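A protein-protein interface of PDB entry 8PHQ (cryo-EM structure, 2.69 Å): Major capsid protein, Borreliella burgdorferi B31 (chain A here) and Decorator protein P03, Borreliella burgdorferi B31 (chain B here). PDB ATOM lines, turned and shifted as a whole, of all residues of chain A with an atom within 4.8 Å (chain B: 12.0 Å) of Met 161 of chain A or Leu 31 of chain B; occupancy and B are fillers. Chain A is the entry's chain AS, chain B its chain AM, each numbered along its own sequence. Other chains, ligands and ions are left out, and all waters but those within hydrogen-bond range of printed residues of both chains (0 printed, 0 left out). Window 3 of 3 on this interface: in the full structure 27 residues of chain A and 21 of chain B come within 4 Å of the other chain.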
ATOM      1  N   GLU A  75     -38.171   8.576 -19.243  1.00  0.00           N
ATOM      2  CA  GLU A  75     -37.181   7.518 -19.363  1.00  0.00           C
ATOM      3  C   GLU A  75     -37.718   6.276 -18.665  1.00  0.00           C
ATOM      4  O   GLU A  75     -38.334   6.376 -17.603  1.00  0.00           O
ATOM      5  CB  GLU A  75     -35.839   7.939 -18.756  1.00  0.00           C
ATOM      6  CG  GLU A  75     -34.748   6.894 -18.870  1.00  0.00           C
ATOM      7  CD  GLU A  75     -33.457   7.331 -18.211  1.00  0.00           C
ATOM      8  OE1 GLU A  75     -33.421   8.445 -17.651  1.00  0.00           O
ATOM      9  OE2 GLU A  75     -32.476   6.559 -18.254  1.00  0.00           O
ATOM     10  N   VAL A  77     -36.936   2.342 -17.228  1.00  0.00           N
ATOM     11  CA  VAL A  77     -35.931   1.407 -16.740  1.00  0.00           C
ATOM     12  C   VAL A  77     -36.626   0.129 -16.295  1.00  0.00           C
ATOM     13  O   VAL A  77     -37.657   0.175 -15.616  1.00  0.00           O
ATOM     14  CB  VAL A  77     -35.101   2.004 -15.585  1.00  0.00           C
ATOM     15  CG1 VAL A  77     -34.144   0.967 -15.034  1.00  0.00           C
ATOM     16  CG2 VAL A  77     -34.338   3.222 -16.062  1.00  0.00           C
ATOM     17  N   TYR A 156     -28.303  -6.301 -10.685  1.00  0.00           N
ATOM     18  CA  TYR A 156     -26.956  -5.916 -10.302  1.00  0.00           C
ATOM     19  C   TYR A 156     -26.909  -5.551  -8.827  1.00  0.00           C
ATOM     20  O   TYR A 156     -27.921  -5.209  -8.213  1.00  0.00           O
ATOM     21  CB  TYR A 156     -26.452  -4.730 -11.136  1.00  0.00           C
ATOM     22  CG  TYR A 156     -26.606  -4.913 -12.625  1.00  0.00           C
ATOM     23  CD1 TYR A 156     -25.819  -5.821 -13.317  1.00  0.00           C
ATOM     24  CD2 TYR A 156     -27.543  -4.181 -13.339  1.00  0.00           C
ATOM     25  CE1 TYR A 156     -25.958  -5.992 -14.678  1.00  0.00           C
ATOM     26  CE2 TYR A 156     -27.688  -4.344 -14.701  1.00  0.00           C
ATOM     27  CZ  TYR A 156     -26.895  -5.251 -15.365  1.00  0.00           C
ATOM     28  OH  TYR A 156     -27.035  -5.420 -16.722  1.00  0.00           O
ATOM     29  N   GLY A 157     -25.704  -5.639  -8.265  1.00  0.00           N
ATOM     30  CA  GLY A 157     -25.422  -5.117  -6.948  1.00  0.00           C
ATOM     31  C   GLY A 157     -24.662  -3.805  -7.021  1.00  0.00           C
ATOM     32  O   GLY A 157     -24.494  -3.202  -8.083  1.00  0.00           O
ATOM     33  N   LEU A 158     -24.198  -3.356  -5.855  1.00  0.00           N
ATOM     34  CA  LEU A 158     -23.439  -2.111  -5.808  1.00  0.00           C
ATOM     35  C   LEU A 158     -22.084  -2.249  -6.488  1.00  0.00           C
ATOM     36  O   LEU A 158     -21.554  -1.264  -7.012  1.00  0.00           O
ATOM     37  CB  LEU A 158     -23.260  -1.657  -4.360  1.00  0.00           C
ATOM     38  CG  LEU A 158     -24.519  -1.180  -3.638  1.00  0.00           C
ATOM     39  CD1 LEU A 158     -24.305  -1.174  -2.135  1.00  0.00           C
ATOM     40  CD2 LEU A 158     -24.917   0.200  -4.129  1.00  0.00           C
ATOM     41  N   LEU A 159     -21.517  -3.453  -6.504  1.00  0.00           N
ATOM     42  CA  LEU A 159     -20.154  -3.641  -6.980  1.00  0.00           C
ATOM     43  C   LEU A 159     -20.060  -3.856  -8.485  1.00  0.00           C
ATOM     44  O   LEU A 159     -19.055  -3.470  -9.091  1.00  0.00           O
ATOM     45  CB  LEU A 159     -19.505  -4.821  -6.254  1.00  0.00           C
ATOM     46  CG  LEU A 159     -17.990  -4.951  -6.405  1.00  0.00           C
ATOM     47  CD1 LEU A 159     -17.296  -3.774  -5.745  1.00  0.00           C
ATOM     48  CD2 LEU A 159     -17.507  -6.260  -5.813  1.00  0.00           C
ATOM     49  N   ASN A 160     -21.072  -4.459  -9.110  1.00  0.00           N
ATOM     50  CA  ASN A 160     -21.030  -4.743 -10.540  1.00  0.00           C
ATOM     51  C   ASN A 160     -22.039  -3.917 -11.331  1.00  0.00           C
ATOM     52  O   ASN A 160     -22.404  -4.299 -12.447  1.00  0.00           O
ATOM     53  CB  ASN A 160     -21.249  -6.234 -10.799  1.00  0.00           C
ATOM     54  CG  ASN A 160     -22.600  -6.723 -10.318  1.00  0.00           C
ATOM     55  OD1 ASN A 160     -23.355  -5.987  -9.687  1.00  0.00           O
ATOM     56  ND2 ASN A 160     -22.917  -7.973 -10.630  1.00  0.00           N
ATOM     57  N   MET A 161     -22.497  -2.802 -10.778  1.00  0.00           N
ATOM     58  CA  MET A 161     -23.398  -1.929 -11.513  1.00  0.00           C
ATOM     59  C   MET A 161     -22.676  -1.360 -12.731  1.00  0.00           C
ATOM     60  O   MET A 161     -21.598  -0.767 -12.584  1.00  0.00           O
ATOM     61  CB  MET A 161     -23.891  -0.797 -10.612  1.00  0.00           C
ATOM     62  CG  MET A 161     -24.980   0.071 -11.218  1.00  0.00           C
ATOM     63  SD  MET A 161     -26.474  -0.848 -11.628  1.00  0.00           S
ATOM     64  CE  MET A 161     -27.219  -1.017 -10.011  1.00  0.00           C
ATOM     65  N   PRO A 162     -23.216  -1.519 -13.932  1.00  0.00           N
ATOM     66  CA  PRO A 162     -22.538  -1.012 -15.127  1.00  0.00           C
ATOM     67  C   PRO A 162     -22.668   0.501 -15.238  1.00  0.00           C
ATOM     68  O   PRO A 162     -23.461   1.139 -14.548  1.00  0.00           O
ATOM     69  CB  PRO A 162     -23.270  -1.720 -16.269  1.00  0.00           C
ATOM     70  CG  PRO A 162     -24.640  -1.927 -15.739  1.00  0.00           C
ATOM     71  CD  PRO A 162     -24.480  -2.200 -14.265  1.00  0.00           C
ATOM     72  N   GLU A 163     -21.852   1.067 -16.128  1.00  0.00           N
ATOM     73  CA  GLU A 163     -21.857   2.503 -16.413  1.00  0.00           C
ATOM     74  C   GLU A 163     -21.567   3.323 -15.156  1.00  0.00           C
ATOM     75  O   GLU A 163     -22.254   4.298 -14.849  1.00  0.00           O
ATOM     76  CB  GLU A 163     -23.182   2.925 -17.052  1.00  0.00           C
ATOM     77  CG  GLU A 163     -23.528   2.159 -18.317  1.00  0.00           C
ATOM     78  CD  GLU A 163     -24.175   3.033 -19.371  1.00  0.00           C
ATOM     79  OE1 GLU A 163     -24.297   4.254 -19.143  1.00  0.00           O
ATOM     80  OE2 GLU A 163     -24.565   2.497 -20.429  1.00  0.00           O
ATOM     81  N   GLN A 164     -20.534   2.915 -14.424  1.00  0.00           N
ATOM     82  CA  GLN A 164     -20.085   3.607 -13.224  1.00  0.00           C
ATOM     83  C   GLN A 164     -18.587   3.855 -13.344  1.00  0.00           C
ATOM     84  O   GLN A 164     -17.949   3.451 -14.320  1.00  0.00           O
ATOM     85  CB  GLN A 164     -20.422   2.803 -11.962  1.00  0.00           C
ATOM     86  CG  GLN A 164     -21.889   2.420 -11.852  1.00  0.00           C
ATOM     87  CD  GLN A 164     -22.789   3.598 -11.546  1.00  0.00           C
ATOM     88  OE1 GLN A 164     -22.319   4.684 -11.213  1.00  0.00           O
ATOM     89  NE2 GLN A 164     -24.093   3.390 -11.666  1.00  0.00           N
ATOM     90  N   LEU A 304     -32.183  -3.275  -7.482  1.00  0.00           N
ATOM     91  CA  LEU A 304     -31.293  -2.138  -7.279  1.00  0.00           C
ATOM     92  C   LEU A 304     -31.294  -1.245  -8.514  1.00  0.00           C
ATOM     93  O   LEU A 304     -31.072  -1.723  -9.630  1.00  0.00           O
ATOM     94  CB  LEU A 304     -29.875  -2.606  -6.961  1.00  0.00           C
ATOM     95  CG  LEU A 304     -28.935  -1.482  -6.527  1.00  0.00           C
ATOM     96  CD1 LEU A 304     -29.464  -0.821  -5.269  1.00  0.00           C
ATOM     97  CD2 LEU A 304     -27.533  -2.008  -6.304  1.00  0.00           C
ATOM     98  N   LEU A 305     -31.536   0.050  -8.314  1.00  0.00           N
ATOM     99  CA  LEU A 305     -31.609   1.027  -9.389  1.00  0.00           C
ATOM    100  C   LEU A 305     -30.645   2.164  -9.089  1.00  0.00           C
ATOM    101  O   LEU A 305     -30.614   2.671  -7.965  1.00  0.00           O
ATOM    102  CB  LEU A 305     -33.037   1.557  -9.538  1.00  0.00           C
ATOM    103  CG  LEU A 305     -33.267   2.725 -10.492  1.00  0.00           C
ATOM    104  CD1 LEU A 305     -33.133   2.264 -11.921  1.00  0.00           C
ATOM    105  CD2 LEU A 305     -34.638   3.327 -10.253  1.00  0.00           C
ATOM    106  N   ALA A 306     -29.854   2.558 -10.082  1.00  0.00           N
ATOM    107  CA  ALA A 306     -28.881   3.621  -9.890  1.00  0.00           C
ATOM    108  C   ALA A 306     -28.831   4.491 -11.134  1.00  0.00           C
ATOM    109  O   ALA A 306     -29.180   4.059 -12.236  1.00  0.00           O
ATOM    110  CB  ALA A 306     -27.487   3.062  -9.580  1.00  0.00           C
ATOM    111  N   THR A 307     -28.403   5.733 -10.943  1.00  0.00           N
ATOM    112  CA  THR A 307     -28.110   6.607 -12.066  1.00  0.00           C
ATOM    113  C   THR A 307     -26.706   6.318 -12.594  1.00  0.00           C
ATOM    114  O   THR A 307     -25.928   5.576 -11.993  1.00  0.00           O
ATOM    115  CB  THR A 307     -28.243   8.073 -11.660  1.00  0.00           C
ATOM    116  OG1 THR A 307     -27.632   8.268 -10.381  1.00  0.00           O
ATOM    117  CG2 THR A 307     -29.704   8.469 -11.571  1.00  0.00           C
ATOM    118  N   ARG A 308     -26.385   6.915 -13.736  1.00  0.00           N
ATOM    119  CA  ARG A 308     -25.092   6.687 -14.363  1.00  0.00           C
ATOM    120  C   ARG A 308     -24.018   7.559 -13.730  1.00  0.00           C
ATOM    121  O   ARG A 308     -24.257   8.723 -13.396  1.00  0.00           O
ATOM    122  CB  ARG A 308     -25.169   6.959 -15.864  1.00  0.00           C
ATOM    123  CG  ARG A 308     -26.322   6.258 -16.556  1.00  0.00           C
ATOM    124  CD  ARG A 308     -26.365   6.583 -18.045  1.00  0.00           C
ATOM    125  NE  ARG A 308     -27.600   6.138 -18.686  1.00  0.00           N
ATOM    126  CZ  ARG A 308     -28.015   4.880 -18.757  1.00  0.00           C
ATOM    127  NH1 ARG A 308     -27.289   3.879 -18.281  1.00  0.00           N
ATOM    128  NH2 ARG A 308     -29.184   4.614 -19.332  1.00  0.00           N
ATOM    129  N   ILE A 311     -21.412   5.830  -8.808  1.00  0.00           N
ATOM    130  CA  ILE A 311     -20.739   4.885  -7.929  1.00  0.00           C
ATOM    131  C   ILE A 311     -19.279   4.792  -8.346  1.00  0.00           C
ATOM    132  O   ILE A 311     -18.973   4.627  -9.535  1.00  0.00           O
ATOM    133  CB  ILE A 311     -21.405   3.496  -7.960  1.00  0.00           C
ATOM    134  CG1 ILE A 311     -22.911   3.616  -7.742  1.00  0.00           C
ATOM    135  CG2 ILE A 311     -20.794   2.591  -6.907  1.00  0.00           C
ATOM    136  CD1 ILE A 311     -23.653   2.317  -7.931  1.00  0.00           C
ATOM    137  N   GLN A 313     -16.095   2.504  -7.979  1.00  0.00           N
ATOM    138  CA  GLN A 313     -15.673   1.140  -7.688  1.00  0.00           C
ATOM    139  C   GLN A 313     -14.175   1.054  -7.948  1.00  0.00           C
ATOM    140  O   GLN A 313     -13.736   1.135  -9.100  1.00  0.00           O
ATOM    141  CB  GLN A 313     -16.439   0.147  -8.558  1.00  0.00           C
ATOM    142  CG  GLN A 313     -17.951   0.288  -8.484  1.00  0.00           C
ATOM    143  CD  GLN A 313     -18.645  -0.175  -9.751  1.00  0.00           C
ATOM    144  OE1 GLN A 313     -17.995  -0.547 -10.727  1.00  0.00           O
ATOM    145  NE2 GLN A 313     -19.971  -0.158  -9.739  1.00  0.00           N
ATOM    146  N   GLN B  27     -37.404   2.464 -25.583  1.00  0.00           N
ATOM    147  CA  GLN B  27     -36.231   1.681 -25.222  1.00  0.00           C
ATOM    148  C   GLN B  27     -36.081   1.661 -23.707  1.00  0.00           C
ATOM    149  O   GLN B  27     -36.192   2.704 -23.053  1.00  0.00           O
ATOM    150  CB  GLN B  27     -34.966   2.241 -25.891  1.00  0.00           C
ATOM    151  CG  GLN B  27     -34.580   3.646 -25.453  1.00  0.00           C
ATOM    152  CD  GLN B  27     -33.371   4.179 -26.193  1.00  0.00           C
ATOM    153  OE1 GLN B  27     -32.773   3.485 -27.013  1.00  0.00           O
ATOM    154  NE2 GLN B  27     -33.003   5.423 -25.905  1.00  0.00           N
ATOM    155  N   ASP B  28     -35.857   0.476 -23.155  1.00  0.00           N
ATOM    156  CA  ASP B  28     -35.628   0.308 -21.727  1.00  0.00           C
ATOM    157  C   ASP B  28     -34.150   0.064 -21.445  1.00  0.00           C
ATOM    158  O   ASP B  28     -33.424  -0.505 -22.265  1.00  0.00           O
ATOM    159  CB  ASP B  28     -36.483  -0.833 -21.166  1.00  0.00           C
ATOM    160  CG  ASP B  28     -36.201  -2.172 -21.829  1.00  0.00           C
ATOM    161  OD1 ASP B  28     -35.409  -2.225 -22.793  1.00  0.00           O
ATOM    162  OD2 ASP B  28     -36.781  -3.183 -21.381  1.00  0.00           O
ATOM    163  N   SER B  29     -33.706   0.519 -20.277  1.00  0.00           N
ATOM    164  CA  SER B  29     -32.317   0.401 -19.861  1.00  0.00           C
ATOM    165  C   SER B  29     -32.266  -0.184 -18.456  1.00  0.00           C
ATOM    166  O   SER B  29     -33.297  -0.404 -17.812  1.00  0.00           O
ATOM    167  CB  SER B  29     -31.606   1.760 -19.916  1.00  0.00           C
ATOM    168  OG  SER B  29     -32.181   2.674 -19.000  1.00  0.00           O
ATOM    169  N   GLY B  30     -31.052  -0.449 -17.984  1.00  0.00           N
ATOM    170  CA  GLY B  30     -30.865  -0.967 -16.644  1.00  0.00           C
ATOM    171  C   GLY B  30     -30.607   0.111 -15.614  1.00  0.00           C
ATOM    172  O   GLY B  30     -30.693  -0.142 -14.409  1.00  0.00           O
ATOM    173  N   LEU B  31     -30.289   1.320 -16.072  1.00  0.00           N
ATOM    174  CA  LEU B  31     -29.972   2.432 -15.189  1.00  0.00           C
ATOM    175  C   LEU B  31     -30.693   3.690 -15.647  1.00  0.00           C
ATOM    176  O   LEU B  31     -31.033   3.849 -16.822  1.00  0.00           O
ATOM    177  CB  LEU B  31     -28.466   2.719 -15.134  1.00  0.00           C
ATOM    178  CG  LEU B  31     -27.540   1.842 -14.290  1.00  0.00           C
ATOM    179  CD1 LEU B  31     -27.330   0.466 -14.906  1.00  0.00           C
ATOM    180  CD2 LEU B  31     -26.219   2.554 -14.086  1.00  0.00           C
ATOM    181  N   LEU B  32     -30.916   4.590 -14.692  1.00  0.00           N
ATOM    182  CA  LEU B  32     -31.441   5.912 -14.995  1.00  0.00           C
ATOM    183  C   LEU B  32     -30.348   6.780 -15.604  1.00  0.00           C
ATOM    184  O   LEU B  32     -29.182   6.703 -15.209  1.00  0.00           O
ATOM    185  CB  LEU B  32     -31.983   6.571 -13.727  1.00  0.00           C
ATOM    186  CG  LEU B  32     -33.348   6.100 -13.226  1.00  0.00           C
ATOM    187  CD1 LEU B  32     -33.698   6.791 -11.920  1.00  0.00           C
ATOM    188  CD2 LEU B  32     -34.417   6.358 -14.270  1.00  0.00           C
ATOM    189  N   SER B  33     -30.729   7.609 -16.570  1.00  0.00           N
ATOM    190  CA  SER B  33     -29.774   8.502 -17.210  1.00  0.00           C
ATOM    191  C   SER B  33     -29.429   9.664 -16.287  1.00  0.00           C
ATOM    192  O   SER B  33     -30.246  10.111 -15.479  1.00  0.00           O
ATOM    193  CB  SER B  33     -30.330   9.034 -18.531  1.00  0.00           C
ATOM    194  OG  SER B  33     -31.317  10.026 -18.307  1.00  0.00           O
ATOM    195  N   ASN B  34     -28.195  10.156 -16.418  1.00  0.00           N
ATOM    196  CA  ASN B  34     -27.692  11.229 -15.563  1.00  0.00           C
ATOM    197  C   ASN B  34     -28.062  12.576 -16.177  1.00  0.00           C
ATOM    198  O   ASN B  34     -27.269  13.233 -16.855  1.00  0.00           O
ATOM    199  CB  ASN B  34     -26.188  11.098 -15.363  1.00  0.00           C
ATOM    200  CG  ASN B  34     -25.743  11.551 -13.987  1.00  0.00           C
ATOM    201  OD1 ASN B  34     -26.539  12.081 -13.209  1.00  0.00           O
ATOM    202  ND2 ASN B  34     -24.468  11.349 -13.679  1.00  0.00           N
ATOM    203  N   SER B  35     -29.302  12.987 -15.930  1.00  0.00           N
ATOM    204  CA  SER B  35     -29.793  14.309 -16.308  1.00  0.00           C
ATOM    205  C   SER B  35     -30.276  14.988 -15.030  1.00  0.00           C
ATOM    206  O   SER B  35     -31.467  14.958 -14.709  1.00  0.00           O
ATOM    207  CB  SER B  35     -30.903  14.211 -17.356  1.00  0.00           C
ATOM    208  OG  SER B  35     -31.968  13.396 -16.897  1.00  0.00           O
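Among the printed residues, pairs that only touch across the chains: Pro 162 of chain A with Leu 31 of chain B (3.1 Å), Val 77 of chain A with Ser 29 of chain B (3.2 Å), Ala 306 of chain A with Leu 31 of chain B (3.3 Å), Thr 307 of chain A with Leu 32 of chain B (3.3 Å), Gln 164 of chain A with Leu 31 of chain B (3.3 Å), Glu 75 of chain A with Leu 32 of chain B (3.4 Å), Val 77 of chain A with Leu 31 of chain B (3.4 Å), Arg 308 of chain A with Ser 33 of chain B (3.5 Å), Arg 308 of chain A with Ser 29 of chain B (3.6 Å), Val 77 of chain A with Leu 32 of chain B (3.6 Å), Met 161 of chain A with Leu 31 of chain B (3.6 Å), Val 77 of chain A with Gly 30 of chain B (3.7 Å), Thr 307 of chain A with Leu 31 of chain B (3.7 Å), Leu 305 of chain A with Leu 32 of chain B (3.96 Å) and Glu 75 of chain A with Ser 29 of chain B (3.97 Å).
The side-chain carboxylate (OE2) of Glu 75 of chain A lies within hydrogen-bond range of the backbone NH (N) of Ser 33 of chain B. The backbone NH (N) of Leu 32 of chain B sits at hydrogen-bond distance from the backbone carbonyl oxygen (O) of Ala 306 of chain A (3.1 Å). The guanidinium group of Arg 308 of chain A is in hydrogen-bond range of the backbone carbonyl oxygen of Leu 31 of chain B, 3.2 Å away. The backbone NH (N) of Arg 308 of chain A lies within hydrogen-bond range of the backbone carbonyl oxygen (O) of Leu 32 of chain B, 3.2 Å away. The backbone carbonyl oxygen of Arg 308 of chain A sits at hydrogen-bond distance from the side-chain amide nitrogen of Asn 34 of chain B. The backbone carbonyl oxygen of Leu 31 of chain B lies close to the side-chain carboxylate of Glu 75 of chain A (3.4 Å).
Along chain B the printed residues that touch a printed residue of chain A span positions 29 to 34. Of the 18 printed residues of chain A, 9 touch a printed residue of chain B. Along chain A the printed residues that touch a printed residue of chain B span positions 75 to 308. Among the printed residues, no Asp or Glu carboxylate lies within 4 Å of a Lys or Arg side-chain nitrogen of the other chain.
The side-chain carboxylate (OE2) of Glu 75 of chain A lies within salt-bridge range of the guanidinium group (NH2) of Arg 308 of chain A, 3.97 Å away. O of Met 161 of chain A sits at hydrogen-bond distance from NE2 of Gln 313 of chain A, at 3.3 Å. OE1 of Glu 163 of chain A is in salt-bridge range of NH1 of Arg 308 of chain A (3.1 Å). NE2 of Gln 164 of chain A lies within hydrogen-bond range of O of Thr 307 of chain A (2.9 Å). OE1 of Gln 164 of chain A is in hydrogen-bond range of N of Ile 311 of chain A, at 2.8 Å. The backbone carbonyl oxygen (O) of Leu 31 of chain B sits at hydrogen-bond distance from the side-chain hydroxyl (OG) of Ser 29 of chain B (2.7 Å).
Printed residues of chain B within 4 Å of Glu 75 of chain A: Ser 29, Leu 31, Leu 32 and Ser 33. Printed residues of chain B within 4 Å of Val 77 of chain A: Ser 29 (3.2 Å), Gly 30 (3.7 Å), Leu 31 (3.4 Å) and Leu 32 (3.6 Å). No residue of chain B comes within 4 Å of Tyr 156 of chain A. No residue of chain B comes within 4 Å of Leu 159 of chain A. No residue of chain B comes within 4 Å of Asn 160 of chain A. Of chain B, only Leu 31 comes within 4 Å of Met 161 of chain A. Pro 162 of chain A touches one residue of chain B. No residue of chain B comes within 4 Å of Glu 163 of chain A. Gln 164 of chain A touches just one residue of chain B: Leu 31. Leu 304 of chain A touches none of the printed residues of chain B. Of chain B, only Leu 32 comes within 4 Å of Leu 305 of chain A. Printed residues of chain B within 4 Å of Ala 306 of chain A: Leu 31 and Leu 32. Arg 308 of chain A touches just these residues of chain B: Ser 29 (3.6 Å), Leu 31 (3.2 Å), Leu 32 (3.2 Å), Ser 33 (3.5 Å) and Asn 34 (2.6 Å). Gln 313 of chain A touches none of the printed residues of chain B. Asp 28 of chain B touches none of the printed residues of chain A. Of the printed residues of chain A, Ser 29 of chain B touches Glu 75 (3.97 Å), Val 77 (3.2 Å) and Arg 308 (3.6 Å). Of the printed residues of chain A, Gly 30 of chain B touches Val 77 (3.7 Å). Leu 31 of chain B touches just these residues of chain A: Glu 75 (3.4 Å), Val 77 (3.4 Å), Met 161 (3.6 Å), Pro 162 (3.1 Å), Gln 164 (3.3 Å), Ala 306 (3.3 Å), Thr 307 (3.7 Å) and Arg 308 (3.2 Å). Of the printed residues of chain A, Ser 33 of chain B touches Glu 75 and Arg 308. The nearest residue of chain B that does not touch Met 161 of chain A is Gly 30 of chain B (5.1 Å). The nearest residue of chain A that does not touch Leu 31 of chain B is Glu 163 of chain A (4.3 Å). The nearest printed residue of chain A that does not touch Asn 34 of chain B is Thr 307 of chain A (4.6 Å).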
